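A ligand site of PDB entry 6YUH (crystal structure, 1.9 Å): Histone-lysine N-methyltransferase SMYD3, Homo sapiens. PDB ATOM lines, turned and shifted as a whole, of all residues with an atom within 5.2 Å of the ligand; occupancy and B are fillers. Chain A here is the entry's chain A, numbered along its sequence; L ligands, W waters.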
ATOM      1  N   ASN A  11      10.270  11.506  -4.539  1.00  0.00           N
ATOM      2  CA  ASN A  11       9.851  12.606  -3.677  1.00  0.00           C
ATOM      3  C   ASN A  11      10.407  12.582  -2.248  1.00  0.00           C
ATOM      4  O   ASN A  11       9.814  13.212  -1.373  1.00  0.00           O
ATOM      5  CB  ASN A  11       8.326  12.683  -3.615  1.00  0.00           C
ATOM      6  CG  ASN A  11       7.688  11.397  -3.104  1.00  0.00           C
ATOM      7  OD1 ASN A  11       8.282  10.640  -2.342  1.00  0.00           O
ATOM      8  ND2 ASN A  11       6.449  11.169  -3.513  1.00  0.00           N
ATOM      9  N   ARG A  12      11.531  11.909  -1.988  1.00  0.00           N
ATOM     10  CA  ARG A  12      12.105  11.960  -0.648  1.00  0.00           C
ATOM     11  C   ARG A  12      13.621  12.038  -0.719  1.00  0.00           C
ATOM     12  O   ARG A  12      14.342  11.422   0.088  1.00  0.00           O
ATOM     13  CB  ARG A  12      11.657  10.763   0.202  1.00  0.00           C
ATOM     14  CG  ARG A  12      11.685   9.416  -0.491  1.00  0.00           C
ATOM     15  CD  ARG A  12      10.651   8.451   0.106  1.00  0.00           C
ATOM     16  NE  ARG A  12       9.292   8.930  -0.122  1.00  0.00           N
ATOM     17  CZ  ARG A  12       8.209   8.404   0.439  1.00  0.00           C
ATOM     18  NH1 ARG A  12       8.320   7.372   1.264  1.00  0.00           N
ATOM     19  NH2 ARG A  12       7.000   8.911   0.177  1.00  0.00           N
ATOM     20  N   GLY A  13      14.144  12.804  -1.668  1.00  0.00           N
ATOM     21  CA  GLY A  13      15.576  12.988  -1.763  1.00  0.00           C
ATOM     22  C   GLY A  13      16.271  11.742  -2.289  1.00  0.00           C
ATOM     23  O   GLY A  13      15.734  10.989  -3.109  1.00  0.00           O
ATOM     24  N   ASN A  14      17.476  11.533  -1.807  1.00  0.00           N
ATOM     25  CA  ASN A  14      18.202  10.311  -2.116  1.00  0.00           C
ATOM     26  C   ASN A  14      17.792   9.197  -1.168  1.00  0.00           C
ATOM     27  O   ASN A  14      17.382   9.444  -0.032  1.00  0.00           O
ATOM     28  CB  ASN A  14      19.715  10.537  -2.015  1.00  0.00           C
ATOM     29  CG  ASN A  14      20.213  11.544  -3.026  1.00  0.00           C
ATOM     30  OD1 ASN A  14      19.836  11.491  -4.195  1.00  0.00           O
ATOM     31  ND2 ASN A  14      21.016  12.481  -2.573  1.00  0.00           N
ATOM     32  N   GLY A  15      17.937   7.969  -1.645  1.00  0.00           N
ATOM     33  CA  GLY A  15      17.624   6.804  -0.845  1.00  0.00           C
ATOM     34  C   GLY A  15      18.486   5.624  -1.227  1.00  0.00           C
ATOM     35  O   GLY A  15      19.429   5.754  -2.017  1.00  0.00           O
ATOM     36  N   TYR A 122      28.022   7.595   0.924  1.00  0.00           N
ATOM     37  CA  TYR A 122      27.429   8.893   1.199  1.00  0.00           C
ATOM     38  C   TYR A 122      28.314   9.550   2.242  1.00  0.00           C
ATOM     39  O   TYR A 122      28.689   8.897   3.215  1.00  0.00           O
ATOM     40  CB  TYR A 122      25.993   8.742   1.718  1.00  0.00           C
ATOM     41  CG  TYR A 122      24.971   9.823   1.362  1.00  0.00           C
ATOM     42  CD1 TYR A 122      24.834  10.310   0.066  1.00  0.00           C
ATOM     43  CD2 TYR A 122      24.084  10.294   2.328  1.00  0.00           C
ATOM     44  CE1 TYR A 122      23.860  11.274  -0.248  1.00  0.00           C
ATOM     45  CE2 TYR A 122      23.117  11.252   2.025  1.00  0.00           C
ATOM     46  CZ  TYR A 122      23.008  11.726   0.750  1.00  0.00           C
ATOM     47  OH  TYR A 122      22.027  12.663   0.491  1.00  0.00           O
ATOM     48  N   ASP A 126      27.436  15.231   1.932  1.00  0.00           N
ATOM     49  CA  ASP A 126      26.235  14.922   1.162  1.00  0.00           C
ATOM     50  C   ASP A 126      24.942  15.010   1.977  1.00  0.00           C
ATOM     51  O   ASP A 126      23.861  15.057   1.378  1.00  0.00           O
ATOM     52  CB  ASP A 126      26.311  13.510   0.587  1.00  0.00           C
ATOM     53  CG  ASP A 126      27.435  13.325  -0.388  1.00  0.00           C
ATOM     54  OD1 ASP A 126      27.685  14.256  -1.187  1.00  0.00           O
ATOM     55  OD2 ASP A 126      28.062  12.239  -0.368  1.00  0.00           O
ATOM     56  N   LEU A 127      25.021  15.022   3.287  1.00  0.00           N
ATOM     57  CA  LEU A 127      23.861  14.736   4.120  1.00  0.00           C
ATOM     58  C   LEU A 127      22.764  15.790   3.937  1.00  0.00           C
ATOM     59  O   LEU A 127      23.045  16.959   3.675  1.00  0.00           O
ATOM     60  CB  LEU A 127      24.258  14.663   5.586  1.00  0.00           C
ATOM     61  CG  LEU A 127      25.130  13.466   5.983  1.00  0.00           C
ATOM     62  CD1 LEU A 127      25.610  13.633   7.420  1.00  0.00           C
ATOM     63  CD2 LEU A 127      24.353  12.138   5.822  1.00  0.00           C
ATOM     64  N   GLU A 128      21.519  15.354   4.095  1.00  0.00           N
ATOM     65  CA  GLU A 128      20.380  16.266   4.046  1.00  0.00           C
ATOM     66  C   GLU A 128      20.409  17.259   5.211  1.00  0.00           C
ATOM     67  O   GLU A 128      20.601  16.888   6.369  1.00  0.00           O
ATOM     68  CB  GLU A 128      19.066  15.471   4.118  1.00  0.00           C
ATOM     69  CG  GLU A 128      17.836  16.379   4.135  1.00  0.00           C
ATOM     70  CD  GLU A 128      17.705  17.181   2.856  1.00  0.00           C
ATOM     71  OE1 GLU A 128      17.498  16.571   1.791  1.00  0.00           O
ATOM     72  OE2 GLU A 128      17.811  18.438   2.905  1.00  0.00           O
ATOM     73  N   ASN A 130      17.768  19.986   5.209  1.00  0.00           N
ATOM     74  CA  ASN A 130      16.385  20.460   5.330  1.00  0.00           C
ATOM     75  C   ASN A 130      16.293  21.946   5.659  1.00  0.00           C
ATOM     76  O   ASN A 130      15.291  22.406   6.207  1.00  0.00           O
ATOM     77  CB  ASN A 130      15.610  19.685   6.400  1.00  0.00           C
ATOM     78  CG  ASN A 130      15.322  18.268   5.984  1.00  0.00           C
ATOM     79  OD1 ASN A 130      14.803  18.018   4.898  1.00  0.00           O
ATOM     80  ND2 ASN A 130      15.669  17.327   6.839  1.00  0.00           N
ATOM     81  N   CYS A 178      18.973  15.800  11.645  1.00  0.00           N
ATOM     82  CA  CYS A 178      18.150  14.796  10.980  1.00  0.00           C
ATOM     83  C   CYS A 178      18.949  13.573  10.530  1.00  0.00           C
ATOM     84  O   CYS A 178      18.401  12.740   9.794  1.00  0.00           O
ATOM     85  CB  CYS A 178      17.437  15.401   9.770  1.00  0.00           C
ATOM     86  SG  CYS A 178      18.537  16.137   8.560  1.00  0.00           S
ATOM     87  N   ASN A 179      20.208  13.429  10.950  1.00  0.00           N
ATOM     88  CA  ASN A 179      21.015  12.281  10.556  1.00  0.00           C
ATOM     89  C   ASN A 179      21.729  11.610  11.728  1.00  0.00           C
ATOM     90  O   ASN A 179      22.642  10.819  11.506  1.00  0.00           O
ATOM     91  CB  ASN A 179      22.042  12.678   9.490  1.00  0.00           C
ATOM     92  CG  ASN A 179      21.385  13.148   8.202  1.00  0.00           C
ATOM     93  OD1 ASN A 179      20.971  12.345   7.368  1.00  0.00           O
ATOM     94  ND2 ASN A 179      21.277  14.467   8.044  1.00  0.00           N
ATOM     95  N   SER A 200      22.749   6.783   6.480  1.00  0.00           N
ATOM     96  CA  SER A 200      21.811   7.904   6.401  1.00  0.00           C
ATOM     97  C   SER A 200      21.153   8.043   5.048  1.00  0.00           C
ATOM     98  O   SER A 200      20.328   8.947   4.875  1.00  0.00           O
ATOM     99  CB  SER A 200      22.514   9.220   6.743  1.00  0.00           C
ATOM    100  OG  SER A 200      22.672   9.366   8.144  1.00  0.00           O
ATOM    101  N   LEU A 201      21.498   7.199   4.081  1.00  0.00           N
ATOM    102  CA  LEU A 201      20.715   7.160   2.847  1.00  0.00           C
ATOM    103  C   LEU A 201      19.350   6.532   3.076  1.00  0.00           C
ATOM    104  O   LEU A 201      18.442   6.776   2.272  1.00  0.00           O
ATOM    105  CB  LEU A 201      21.481   6.390   1.752  1.00  0.00           C
ATOM    106  CG  LEU A 201      22.475   7.226   0.930  1.00  0.00           C
ATOM    107  CD1 LEU A 201      23.351   6.336   0.050  1.00  0.00           C
ATOM    108  CD2 LEU A 201      21.752   8.256   0.089  1.00  0.00           C
ATOM    109  N   LEU A 202      19.172   5.763   4.145  1.00  0.00           N
ATOM    110  CA  LEU A 202      17.912   5.046   4.348  1.00  0.00           C
ATOM    111  C   LEU A 202      16.783   6.007   4.713  1.00  0.00           C
ATOM    112  O   LEU A 202      16.863   6.731   5.719  1.00  0.00           O
ATOM    113  CB  LEU A 202      18.071   3.977   5.429  1.00  0.00           C
ATOM    114  CG  LEU A 202      18.968   2.765   5.118  1.00  0.00           C
ATOM    115  CD1 LEU A 202      19.545   2.198   6.382  1.00  0.00           C
ATOM    116  CD2 LEU A 202      18.200   1.689   4.366  1.00  0.00           C
ATOM    117  N   ASN A 203      15.727   6.009   3.904  1.00  0.00           N
ATOM    118  CA  ASN A 203      14.545   6.765   4.261  1.00  0.00           C
ATOM    119  C   ASN A 203      13.719   5.989   5.279  1.00  0.00           C
ATOM    120  O   ASN A 203      13.957   4.819   5.542  1.00  0.00           O
ATOM    121  CB  ASN A 203      13.716   7.100   3.018  1.00  0.00           C
ATOM    122  CG  ASN A 203      14.349   8.207   2.193  1.00  0.00           C
ATOM    123  OD1 ASN A 203      14.786   9.236   2.730  1.00  0.00           O
ATOM    124  ND2 ASN A 203      14.409   8.000   0.895  1.00  0.00           N
ATOM    125  N   HIS A 204      12.730   6.673   5.844  1.00  0.00           N
ATOM    126  CA  HIS A 204      11.948   6.134   6.951  1.00  0.00           C
ATOM    127  C   HIS A 204      10.663   5.468   6.480  1.00  0.00           C
ATOM    128  O   HIS A 204      10.065   5.855   5.472  1.00  0.00           O
ATOM    129  CB  HIS A 204      11.591   7.255   7.925  1.00  0.00           C
ATOM    130  CG  HIS A 204      10.471   6.904   8.854  1.00  0.00           C
ATOM    131  ND1 HIS A 204      10.676   6.324  10.090  1.00  0.00           N
ATOM    132  CD2 HIS A 204       9.120   7.027   8.725  1.00  0.00           C
ATOM    133  CE1 HIS A 204       9.515   6.127  10.684  1.00  0.00           C
ATOM    134  NE2 HIS A 204       8.550   6.542   9.874  1.00  0.00           N
ATOM    135  N   SER A 205      10.223   4.482   7.258  1.00  0.00           N
ATOM    136  CA  SER A 205       8.918   3.866   7.155  1.00  0.00           C
ATOM    137  C   SER A 205       8.459   3.432   8.542  1.00  0.00           C
ATOM    138  O   SER A 205       9.246   2.862   9.295  1.00  0.00           O
ATOM    139  CB  SER A 205       8.927   2.636   6.233  1.00  0.00           C
ATOM    140  OG  SER A 205       7.629   2.082   6.161  1.00  0.00           O
ATOM    141  N   TYR A 237      12.727   5.189  11.877  1.00  0.00           N
ATOM    142  CA  TYR A 237      13.507   6.130  12.675  1.00  0.00           C
ATOM    143  C   TYR A 237      13.034   6.185  14.125  1.00  0.00           C
ATOM    144  O   TYR A 237      13.778   6.674  14.987  1.00  0.00           O
ATOM    145  CB  TYR A 237      13.401   7.555  12.099  1.00  0.00           C
ATOM    146  CG  TYR A 237      13.986   7.797  10.708  1.00  0.00           C
ATOM    147  CD1 TYR A 237      14.662   6.809  10.023  1.00  0.00           C
ATOM    148  CD2 TYR A 237      13.842   9.034  10.114  1.00  0.00           C
ATOM    149  CE1 TYR A 237      15.194   7.058   8.745  1.00  0.00           C
ATOM    150  CE2 TYR A 237      14.369   9.302   8.850  1.00  0.00           C
ATOM    151  CZ  TYR A 237      15.031   8.306   8.171  1.00  0.00           C
ATOM    152  OH  TYR A 237      15.545   8.582   6.920  1.00  0.00           O
ATOM    153  N   GLN A 254      11.777  16.916  13.831  1.00  0.00           N
ATOM    154  CA  GLN A 254      13.181  16.534  13.692  1.00  0.00           C
ATOM    155  C   GLN A 254      13.589  16.289  12.259  1.00  0.00           C
ATOM    156  O   GLN A 254      14.759  16.496  11.899  1.00  0.00           O
ATOM    157  CB  GLN A 254      13.472  15.272  14.512  1.00  0.00           C
ATOM    158  CG  GLN A 254      14.947  14.885  14.586  1.00  0.00           C
ATOM    159  CD  GLN A 254      15.207  13.658  15.446  1.00  0.00           C
ATOM    160  OE1 GLN A 254      14.338  13.236  16.209  1.00  0.00           O
ATOM    161  NE2 GLN A 254      16.398  13.094  15.323  1.00  0.00           N
ATOM    162  N   TYR A 255      12.662  15.803  11.425  1.00  0.00           N
ATOM    163  CA  TYR A 255      13.004  15.323  10.097  1.00  0.00           C
ATOM    164  C   TYR A 255      12.344  16.113   8.986  1.00  0.00           C
ATOM    165  O   TYR A 255      12.632  15.854   7.810  1.00  0.00           O
ATOM    166  CB  TYR A 255      12.648  13.834   9.965  1.00  0.00           C
ATOM    167  CG  TYR A 255      13.448  12.941  10.880  1.00  0.00           C
ATOM    168  CD1 TYR A 255      14.769  12.634  10.595  1.00  0.00           C
ATOM    169  CD2 TYR A 255      12.890  12.419  12.047  1.00  0.00           C
ATOM    170  CE1 TYR A 255      15.502  11.815  11.428  1.00  0.00           C
ATOM    171  CE2 TYR A 255      13.624  11.616  12.888  1.00  0.00           C
ATOM    172  CZ  TYR A 255      14.923  11.310  12.580  1.00  0.00           C
ATOM    173  OH  TYR A 255      15.664  10.502  13.414  1.00  0.00           O
ATOM    174  N   CYS A 256      11.485  17.081   9.311  1.00  0.00           N
ATOM    175  CA  CYS A 256      10.827  17.934   8.318  1.00  0.00           C
ATOM    176  C   CYS A 256      10.176  17.122   7.202  1.00  0.00           C
ATOM    177  O   CYS A 256      10.393  17.391   6.010  1.00  0.00           O
ATOM    178  CB  CYS A 256      11.822  18.942   7.733  1.00  0.00           C
ATOM    179  SG  CYS A 256      12.513  20.118   8.919  1.00  0.00           S
ATOM    180  N   PHE A 257       9.359  16.128   7.558  1.00  0.00           N
ATOM    181  CA  PHE A 257       8.515  15.518   6.542  1.00  0.00           C
ATOM    182  C   PHE A 257       7.220  14.987   7.155  1.00  0.00           C
ATOM    183  O   PHE A 257       7.103  14.810   8.363  1.00  0.00           O
ATOM    184  CB  PHE A 257       9.248  14.416   5.737  1.00  0.00           C
ATOM    185  CG  PHE A 257       9.432  13.100   6.465  1.00  0.00           C
ATOM    186  CD1 PHE A 257      10.581  12.865   7.230  1.00  0.00           C
ATOM    187  CD2 PHE A 257       8.510  12.064   6.322  1.00  0.00           C
ATOM    188  CE1 PHE A 257      10.764  11.655   7.879  1.00  0.00           C
ATOM    189  CE2 PHE A 257       8.700  10.850   6.964  1.00  0.00           C
ATOM    190  CZ  PHE A 257       9.830  10.643   7.739  1.00  0.00           C
ATOM    191  N   GLU A 258       6.245  14.791   6.283  1.00  0.00           N
ATOM    192  CA  GLU A 258       4.941  14.255   6.627  1.00  0.00           C
ATOM    193  C   GLU A 258       4.882  12.839   6.072  1.00  0.00           C
ATOM    194  O   GLU A 258       5.124  12.640   4.877  1.00  0.00           O
ATOM    195  CB  GLU A 258       3.815  15.121   6.048  1.00  0.00           C
ATOM    196  CG  GLU A 258       4.177  16.620   5.902  1.00  0.00           C
ATOM    197  CD  GLU A 258       3.942  17.377   7.188  1.00  0.00           C
ATOM    198  OE1 GLU A 258       3.262  16.803   8.049  1.00  0.00           O
ATOM    199  OE2 GLU A 258       4.427  18.529   7.344  1.00  0.00           O
ATOM    200  N   CYS A 259       4.610  11.874   6.932  1.00  0.00           N
ATOM    201  CA  CYS A 259       4.679  10.482   6.523  1.00  0.00           C
ATOM    202  C   CYS A 259       3.414  10.086   5.772  1.00  0.00           C
ATOM    203  O   CYS A 259       2.303  10.262   6.285  1.00  0.00           O
ATOM    204  CB  CYS A 259       4.882   9.551   7.719  1.00  0.00           C
ATOM    205  SG  CYS A 259       5.285   7.867   7.207  1.00  0.00           S
HETATM  206  N1  LIG L   1      16.420  11.248   1.743  1.00  0.00           N
HETATM  207  C1  LIG L   1      17.602  11.577   2.528  1.00  0.00           C
HETATM  208  C2  LIG L   1      18.686  12.231   1.674  1.00  0.00           C
HETATM  209  O1  LIG L   1      18.446  12.618   0.519  1.00  0.00           O
HETATM  210  O2  LIG L   1      19.830  12.398   2.131  1.00  0.00           O
HETATM  211  C3  LIG L   1      18.144  10.318   3.214  1.00  0.00           C
HETATM  212  C4  LIG L   1      17.488  10.001   4.562  1.00  0.00           C
HETATM  213  S1  LIG L   1      17.992  11.196   5.824  1.00  0.00           S
HETATM  214  C5  LIG L   1      18.577  10.122   7.139  1.00  0.00           C
HETATM  215  C6  LIG L   1      16.429  11.744   6.553  1.00  0.00           C
HETATM  216  C7  LIG L   1      15.695  12.743   5.674  1.00  0.00           C
HETATM  217  O3  LIG L   1      15.175  12.076   4.527  1.00  0.00           O
HETATM  218  C8  LIG L   1      14.493  13.381   6.360  1.00  0.00           C
HETATM  219  O4  LIG L   1      14.826  14.506   7.150  1.00  0.00           O
HETATM  220  C9  LIG L   1      13.610  13.729   5.178  1.00  0.00           C
HETATM  221  O5  LIG L   1      14.137  14.865   4.522  1.00  0.00           O
HETATM  222  C10 LIG L   1      13.864  12.562   4.235  1.00  0.00           C
HETATM  223  N2  LIG L   1      12.946  11.433   4.430  1.00  0.00           N
HETATM  224  C11 LIG L   1      13.261  10.276   5.088  1.00  0.00           C
HETATM  225  N3  LIG L   1      12.191   9.460   5.064  1.00  0.00           N
HETATM  226  C12 LIG L   1      11.184  10.070   4.403  1.00  0.00           C
HETATM  227  C13 LIG L   1       9.884   9.676   4.078  1.00  0.00           C
HETATM  228  N4  LIG L   1       9.406   8.486   4.447  1.00  0.00           N
HETATM  229  N5  LIG L   1       9.072  10.520   3.367  1.00  0.00           N
HETATM  230  C14 LIG L   1       9.545  11.752   2.969  1.00  0.00           C
HETATM  231  N6  LIG L   1      10.838  12.143   3.288  1.00  0.00           N
HETATM  232  C15 LIG L   1      11.651  11.317   3.989  1.00  0.00           C
HETATM  233  O   HOH W   1      12.274  17.017   4.155  1.00  0.00           O
HETATM  234  O   HOH W   2       6.587   7.527   4.281  1.00  0.00           O
HETATM  235  O   HOH W   3       6.310  10.554   3.281  1.00  0.00           O
HETATM  236  O   HOH W   4      19.217  15.186  -0.255  1.00  0.00           O
HETATM  237  O   HOH W   5      11.213  14.900   2.309  1.00  0.00           O
HETATM  238  O   HOH W   6       7.642  12.619   0.334  1.00  0.00           O
HETATM  239  O   HOH W   7      15.665  14.116   1.730  1.00  0.00           O
HETATM  240  O   HOH W   8      21.085  12.743   4.849  1.00  0.00           O
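The backbone carbonyl oxygen (O) of His 204 is in hydrogen-bond range of a nitrogen (N4) of the ligand, at 2.9 Å.
The backbone carbonyl oxygen (O) of Arg 12 sits at hydrogen-bond distance from a nitrogen (N1) of the ligand (2.7 Å).
An oxygen (O4) of the ligand lies within hydrogen-bond range of the side-chain amide nitrogen of Asn 130 (3.0 Å).
An oxygen (O4) of the ligand is in hydrogen-bond range of the backbone carbonyl oxygen (O) of Tyr 255, at 2.7 Å.
The backbone NH (N) of His 204 sits at hydrogen-bond distance from a nitrogen (N3) of the ligand.
The backbone carbonyl oxygen of Asn 14 is in hydrogen-bond range of a nitrogen (N1) of the ligand.
The backbone NH of Asn 14 sits at hydrogen-bond distance from an oxygen (O1) of the ligand (2.7 Å).
The side-chain amide oxygen (OD1) of Asn 203 lies within hydrogen-bond range of a nitrogen (N1) of the ligand, 2.8 Å away.
An oxygen (O2) of the ligand is in hydrogen-bond range of the side-chain hydroxyl (OH) of Tyr 122, 2.8 Å away.
OH of Tyr 122 is in hydrogen-bond range of O of Asp 126.
The side-chain hydroxyl of Tyr 237 is in hydrogen-bond range of the backbone carbonyl oxygen of Leu 202 (2.6 Å).
The backbone carbonyl oxygen of Asn 14 lies within hydrogen-bond range of the side-chain amide nitrogen of Asn 203, at 3.4 Å.
ND2 of Asn 130 is in hydrogen-bond range of SG of Cys 178.
The backbone carbonyl oxygen of Glu 128 is in hydrogen-bond range of the side-chain sulfur of Cys 178 (3.1 Å).
The side-chain amide nitrogen (ND2) of Asn 179 lies within hydrogen-bond range of the side-chain sulfur (SG) of Cys 178, 3.3 Å away.
N of Asn 130 lies within hydrogen-bond range of OE2 of Glu 128 (2.8 Å).
The backbone NH (N) of Tyr 237 lies within hydrogen-bond range of a ring nitrogen (ND1) of His 204, 2.9 Å away.
S1 of the ligand lies close to OD1 of Asn 179 (3.5 Å).
S1 of the ligand lies close to O of Ser 200 (3.4 Å).
OH of Tyr 237 sits close to S1 of the ligand, at 3.7 Å.
Gly 13 touches the ligand (C to O1, 3.7 Å).
CB of Glu 128 touches O2 of the ligand, at 3.7 Å.
O of Cys 178 touches C5 of the ligand (3.7 Å).
Leu 201 touches the ligand.
O of Leu 202 touches C4 of the ligand (3.5 Å).
Phe 257 touches the ligand (CE2 to C13, 3.3 Å).
16 residues have an atom within 4 Å of the ligand: Arg 12, Gly 13, Asn 14, Tyr 122, Glu 128, Asn 130, Cys 178, Asn 179, Ser 200, Leu 201, Leu 202, Asn 203, His 204, Tyr 237, Tyr 255 and Phe 257.
Water W3 bridges a nitrogen (N5) of the ligand (2.8 Å) and the backbone carbonyl oxygen (O) of Glu 258 (2.9 Å).
Water W4 bridges O1 of the ligand and OE1 of Glu 128.
Water W1 lies within hydrogen-bond range of the backbone carbonyl oxygen (O) of Cys 256 (2.7 Å), the side-chain amide oxygen (OD1) of Asn 130 (2.8 Å) and an oxygen (O5) of the ligand (2.9 Å).
Water W7 lies within hydrogen-bond range of a nitrogen (N1) of the ligand (3.0 Å), the side-chain carboxylate of Glu 128 (3.1 Å) and the backbone carbonyl oxygen of Arg 12 (3.4 Å).
Water W2 lies within hydrogen-bond range of a nitrogen (N4) of the ligand (3.0 Å) and the guanidinium group of Arg 12 (3.5 Å).
Water W8 lies within hydrogen-bond range of the side-chain amide oxygen of Asn 179 (2.6 Å), the backbone NH of Glu 128 (2.8 Å) and an oxygen (O2) of the ligand (3.0 Å).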
